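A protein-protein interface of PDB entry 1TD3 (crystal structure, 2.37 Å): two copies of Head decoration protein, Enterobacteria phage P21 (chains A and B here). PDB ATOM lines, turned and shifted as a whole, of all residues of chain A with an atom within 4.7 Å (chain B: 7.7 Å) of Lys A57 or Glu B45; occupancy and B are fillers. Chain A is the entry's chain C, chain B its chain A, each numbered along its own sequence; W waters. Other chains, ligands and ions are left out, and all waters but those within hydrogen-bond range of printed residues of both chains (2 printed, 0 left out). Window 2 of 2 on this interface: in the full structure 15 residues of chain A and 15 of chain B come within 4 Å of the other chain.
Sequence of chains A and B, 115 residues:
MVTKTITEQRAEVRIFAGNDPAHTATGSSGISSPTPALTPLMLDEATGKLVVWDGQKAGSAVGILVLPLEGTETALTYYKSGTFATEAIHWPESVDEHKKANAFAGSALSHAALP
NZ of Lys A57 is in salt-bridge range of OE2 of Glu B45 (3.7 Å).
The side-chain carboxylate (OD1) of Asp B44 is in hydrogen-bond range of the backbone NH (N) of Thr B47. OG1 of Thr B47 sits at hydrogen-bond distance from N of Lys B49 (3.1 Å). The indole nitrogen (NE1) of Trp A53 sits at hydrogen-bond distance from the backbone carbonyl oxygen (O) of Lys A57. NZ of Lys A99 is in hydrogen-bond range of O of Gln A56 (2.8 Å).
Among the printed residues, pairs that only touch across the chains: Ala A58 with Leu B43 (3.2 Å), Ala A58 with Gly B48 (3.3 Å), Gly A59 with Leu B43 (3.5 Å) and Lys A99 with Thr B47 (3.8 Å).
Lys A57 touches just one residue of chain B: Glu B45 (3.4 Å). Printed residues of chain B within 4 Å of Lys A99: Thr B47. Of the printed residues of chain A, Glu B45 touches Lys A57 (3.4 Å). Printed residues of chain A within 4 Å of Thr B47: Lys A99 (3.8 Å). Of the printed residues of chain A, Gly B48 touches Ala A58. The nearest residue of chain B that does not touch Lys A57 is Gly B48 (6.0 Å). The nearest printed residue of chain A that does not touch Glu B45 is Lys A99 (4.8 Å).
Of the 9 printed residues of chain A, 4 touch a printed residue of chain B. Printed residues of chain A that touch a printed residue of chain B: Lys A57, Ala A58, Gly A59 and Lys A99. Hydrophobic or aromatic side chains of chain A that line the printed part of chain B: Ala A58. Along chain A the printed residues that touch a printed residue of chain B span positions 57 to 99. Of the 9 printed residues of chain B, 4 touch a printed residue of chain A. Printed residues of chain B that touch a printed residue of chain A: Leu B43, Glu B45, Thr B47 and Gly B48.
No position is printed for both chains. Of the 5 pairs that touch across the chains among the printed residues, none has its exchanged pair printed and touching as well.
Water W1 lies within hydrogen-bond range of N of Ala A58 (2.8 Å) and O of Glu B45 (3.3 Å). Water W2 bridges the side-chain carboxylate (OE1) of Glu B45 (3.1 Å) and the backbone carbonyl oxygen (O) of Ala A58 (3.3 Å).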
ATOM      1  N   TRP A  53       7.011   7.794  -5.880  1.00  0.00           N
ATOM      2  CA  TRP A  53       6.969   6.786  -4.837  1.00  0.00           C
ATOM      3  C   TRP A  53       6.345   7.454  -3.616  1.00  0.00           C
ATOM      4  O   TRP A  53       6.787   8.534  -3.206  1.00  0.00           O
ATOM      5  CB  TRP A  53       8.386   6.333  -4.503  1.00  0.00           C
ATOM      6  CG  TRP A  53       8.465   5.256  -3.475  1.00  0.00           C
ATOM      7  CD1 TRP A  53       7.882   4.018  -3.534  1.00  0.00           C
ATOM      8  CD2 TRP A  53       9.215   5.288  -2.259  1.00  0.00           C
ATOM      9  NE1 TRP A  53       8.230   3.278  -2.429  1.00  0.00           N
ATOM     10  CE2 TRP A  53       9.050   4.033  -1.632  1.00  0.00           C
ATOM     11  CE3 TRP A  53      10.014   6.257  -1.637  1.00  0.00           C
ATOM     12  CZ2 TRP A  53       9.659   3.720  -0.413  1.00  0.00           C
ATOM     13  CZ3 TRP A  53      10.614   5.949  -0.428  1.00  0.00           C
ATOM     14  CH2 TRP A  53      10.433   4.687   0.173  1.00  0.00           C
ATOM     15  N   ASP A  54       5.323   6.829  -3.030  1.00  0.00           N
ATOM     16  CA  ASP A  54       4.665   7.424  -1.863  1.00  0.00           C
ATOM     17  C   ASP A  54       5.354   7.115  -0.536  1.00  0.00           C
ATOM     18  O   ASP A  54       5.012   7.695   0.497  1.00  0.00           O
ATOM     19  CB  ASP A  54       3.189   7.007  -1.790  1.00  0.00           C
ATOM     20  CG  ASP A  54       3.004   5.505  -1.732  1.00  0.00           C
ATOM     21  OD1 ASP A  54       3.798   4.832  -1.046  1.00  0.00           O
ATOM     22  OD2 ASP A  54       2.053   4.997  -2.361  1.00  0.00           O
ATOM     23  N   GLY A  55       6.323   6.206  -0.563  1.00  0.00           N
ATOM     24  CA  GLY A  55       7.039   5.865   0.654  1.00  0.00           C
ATOM     25  C   GLY A  55       6.320   4.890   1.578  1.00  0.00           C
ATOM     26  O   GLY A  55       6.836   4.572   2.652  1.00  0.00           O
ATOM     27  N   GLN A  56       5.150   4.401   1.163  1.00  0.00           N
ATOM     28  CA  GLN A  56       4.368   3.464   1.972  1.00  0.00           C
ATOM     29  C   GLN A  56       4.910   2.044   2.045  1.00  0.00           C
ATOM     30  O   GLN A  56       4.672   1.336   3.026  1.00  0.00           O
ATOM     31  CB  GLN A  56       2.917   3.412   1.476  1.00  0.00           C
ATOM     32  CG  GLN A  56       2.143   4.710   1.687  1.00  0.00           C
ATOM     33  CD  GLN A  56       2.411   5.324   3.052  1.00  0.00           C
ATOM     34  OE1 GLN A  56       2.248   4.672   4.085  1.00  0.00           O
ATOM     35  NE2 GLN A  56       2.832   6.587   3.061  1.00  0.00           N
ATOM     36  N   LYS A  57       5.627   1.618   1.010  1.00  0.00           N
ATOM     37  CA  LYS A  57       6.181   0.271   0.977  1.00  0.00           C
ATOM     38  C   LYS A  57       7.634   0.195   0.515  1.00  0.00           C
ATOM     39  O   LYS A  57       8.018   0.814  -0.474  1.00  0.00           O
ATOM     40  CB  LYS A  57       5.342  -0.620   0.062  1.00  0.00           C
ATOM     41  CG  LYS A  57       4.109  -1.206   0.698  1.00  0.00           C
ATOM     42  CD  LYS A  57       3.493  -2.242  -0.222  1.00  0.00           C
ATOM     43  CE  LYS A  57       4.500  -3.337  -0.565  1.00  0.00           C
ATOM     44  NZ  LYS A  57       3.945  -4.353  -1.511  1.00  0.00           N
ATOM     45  N   ALA A  58       8.432  -0.576   1.241  1.00  0.00           N
ATOM     46  CA  ALA A  58       9.825  -0.777   0.887  1.00  0.00           C
ATOM     47  C   ALA A  58       9.798  -1.703  -0.328  1.00  0.00           C
ATOM     48  O   ALA A  58       8.991  -2.633  -0.380  1.00  0.00           O
ATOM     49  CB  ALA A  58      10.555  -1.445   2.022  1.00  0.00           C
ATOM     50  N   GLY A  59      10.658  -1.441  -1.311  1.00  0.00           N
ATOM     51  CA  GLY A  59      10.706  -2.295  -2.490  1.00  0.00           C
ATOM     52  C   GLY A  59       9.729  -1.901  -3.580  1.00  0.00           C
ATOM     53  O   GLY A  59       9.667  -2.541  -4.634  1.00  0.00           O
ATOM     54  N   SER A  60       8.974  -0.836  -3.333  1.00  0.00           N
ATOM     55  CA  SER A  60       7.976  -0.352  -4.282  1.00  0.00           C
ATOM     56  C   SER A  60       8.569   0.625  -5.307  1.00  0.00           C
ATOM     57  O   SER A  60       8.081   0.718  -6.431  1.00  0.00           O
ATOM     58  CB  SER A  60       6.814   0.329  -3.518  1.00  0.00           C
ATOM     59  OG  SER A  60       5.911   0.957  -4.406  1.00  0.00           O
ATOM     60  N   LYS A  99      11.983   2.006   5.278  1.00  0.00           N
ATOM     61  CA  LYS A  99      11.373   1.869   3.963  1.00  0.00           C
ATOM     62  C   LYS A  99      12.133   2.729   2.965  1.00  0.00           C
ATOM     63  O   LYS A  99      12.105   2.475   1.756  1.00  0.00           O
ATOM     64  CB  LYS A  99       9.912   2.304   4.005  1.00  0.00           C
ATOM     65  CG  LYS A  99       9.056   1.457   4.939  1.00  0.00           C
ATOM     66  CD  LYS A  99       7.591   1.861   4.861  1.00  0.00           C
ATOM     67  CE  LYS A  99       6.731   0.977   5.766  1.00  0.00           C
ATOM     68  NZ  LYS A  99       5.296   1.388   5.741  1.00  0.00           N
ATOM     69  N   MET B  42      14.276 -11.290   2.069  1.00  0.00           N
ATOM     70  CA  MET B  42      12.993 -10.787   1.610  1.00  0.00           C
ATOM     71  C   MET B  42      12.667  -9.533   2.407  1.00  0.00           C
ATOM     72  O   MET B  42      13.284  -9.265   3.437  1.00  0.00           O
ATOM     73  CB  MET B  42      11.897 -11.828   1.853  1.00  0.00           C
ATOM     74  CG  MET B  42      11.466 -11.946   3.320  1.00  0.00           C
ATOM     75  SD  MET B  42      10.130 -13.149   3.600  1.00  0.00           S
ATOM     76  CE  MET B  42       8.715 -12.186   3.095  1.00  0.00           C
ATOM     77  N   LEU B  43      11.700  -8.760   1.933  1.00  0.00           N
ATOM     78  CA  LEU B  43      11.294  -7.564   2.658  1.00  0.00           C
ATOM     79  C   LEU B  43      10.155  -7.918   3.627  1.00  0.00           C
ATOM     80  O   LEU B  43       9.323  -8.782   3.334  1.00  0.00           O
ATOM     81  CB  LEU B  43      10.809  -6.480   1.688  1.00  0.00           C
ATOM     82  CG  LEU B  43      11.843  -5.780   0.797  1.00  0.00           C
ATOM     83  CD1 LEU B  43      11.139  -4.959  -0.269  1.00  0.00           C
ATOM     84  CD2 LEU B  43      12.733  -4.894   1.654  1.00  0.00           C
ATOM     85  N   ASP B  44      10.136  -7.269   4.787  1.00  0.00           N
ATOM     86  CA  ASP B  44       9.070  -7.485   5.760  1.00  0.00           C
ATOM     87  C   ASP B  44       8.068  -6.369   5.495  1.00  0.00           C
ATOM     88  O   ASP B  44       8.354  -5.201   5.750  1.00  0.00           O
ATOM     89  CB  ASP B  44       9.589  -7.358   7.186  1.00  0.00           C
ATOM     90  CG  ASP B  44       8.507  -7.650   8.228  1.00  0.00           C
ATOM     91  OD1 ASP B  44       7.353  -7.199   8.047  1.00  0.00           O
ATOM     92  OD2 ASP B  44       8.814  -8.321   9.233  1.00  0.00           O
ATOM     93  N   GLU B  45       6.900  -6.735   4.978  1.00  0.00           N
ATOM     94  CA  GLU B  45       5.852  -5.772   4.646  1.00  0.00           C
ATOM     95  C   GLU B  45       5.508  -4.803   5.773  1.00  0.00           C
ATOM     96  O   GLU B  45       5.407  -3.591   5.552  1.00  0.00           O
ATOM     97  CB  GLU B  45       4.595  -6.522   4.207  1.00  0.00           C
ATOM     98  CG  GLU B  45       4.232  -6.328   2.744  1.00  0.00           C
ATOM     99  CD  GLU B  45       3.736  -4.927   2.449  1.00  0.00           C
ATOM    100  OE1 GLU B  45       4.477  -3.965   2.728  1.00  0.00           O
ATOM    101  OE2 GLU B  45       2.604  -4.788   1.939  1.00  0.00           O
ATOM    102  N   ALA B  46       5.338  -5.329   6.978  1.00  0.00           N
ATOM    103  CA  ALA B  46       4.992  -4.486   8.115  1.00  0.00           C
ATOM    104  C   ALA B  46       6.026  -3.399   8.401  1.00  0.00           C
ATOM    105  O   ALA B  46       5.675  -2.238   8.602  1.00  0.00           O
ATOM    106  CB  ALA B  46       4.792  -5.353   9.357  1.00  0.00           C
ATOM    107  N   THR B  47       7.299  -3.771   8.406  1.00  0.00           N
ATOM    108  CA  THR B  47       8.361  -2.818   8.724  1.00  0.00           C
ATOM    109  C   THR B  47       9.128  -2.237   7.546  1.00  0.00           C
ATOM    110  O   THR B  47       9.647  -1.129   7.628  1.00  0.00           O
ATOM    111  CB  THR B  47       9.395  -3.460   9.647  1.00  0.00           C
ATOM    112  OG1 THR B  47      10.031  -4.548   8.956  1.00  0.00           O
ATOM    113  CG2 THR B  47       8.730  -3.969  10.923  1.00  0.00           C
ATOM    114  N   GLY B  48       9.220  -2.988   6.458  1.00  0.00           N
ATOM    115  CA  GLY B  48       9.960  -2.504   5.311  1.00  0.00           C
ATOM    116  C   GLY B  48      11.424  -2.879   5.459  1.00  0.00           C
ATOM    117  O   GLY B  48      12.274  -2.439   4.694  1.00  0.00           O
ATOM    118  N   LYS B  49      11.712  -3.696   6.458  1.00  0.00           N
ATOM    119  CA  LYS B  49      13.070  -4.141   6.714  1.00  0.00           C
ATOM    120  C   LYS B  49      13.322  -5.465   6.017  1.00  0.00           C
ATOM    121  O   LYS B  49      12.386  -6.177   5.659  1.00  0.00           O
ATOM    122  CB  LYS B  49      13.303  -4.337   8.209  1.00  0.00           C
ATOM    123  CG  LYS B  49      13.294  -3.059   9.036  1.00  0.00           C
ATOM    124  CD  LYS B  49      13.633  -3.385  10.491  1.00  0.00           C
ATOM    125  CE  LYS B  49      13.838  -2.130  11.329  1.00  0.00           C
ATOM    126  NZ  LYS B  49      14.283  -2.472  12.709  1.00  0.00           N
ATOM    127  N   VAL B  51      14.634  -9.295   5.927  1.00  0.00           N
ATOM    128  CA  VAL B  51      14.705 -10.429   6.826  1.00  0.00           C
ATOM    129  C   VAL B  51      14.910 -11.647   5.941  1.00  0.00           C
ATOM    130  O   VAL B  51      14.920 -11.538   4.711  1.00  0.00           O
ATOM    131  CB  VAL B  51      13.380 -10.576   7.658  1.00  0.00           C
ATOM    132  CG1 VAL B  51      13.145  -9.320   8.506  1.00  0.00           C
ATOM    133  CG2 VAL B  51      12.204 -10.779   6.735  1.00  0.00           C
HETATM  134  O   HOH W   1       7.296  -2.124   3.293  1.00  0.00           O
HETATM  135  O   HOH W   2       7.093  -4.753   1.201  1.00  0.00           O
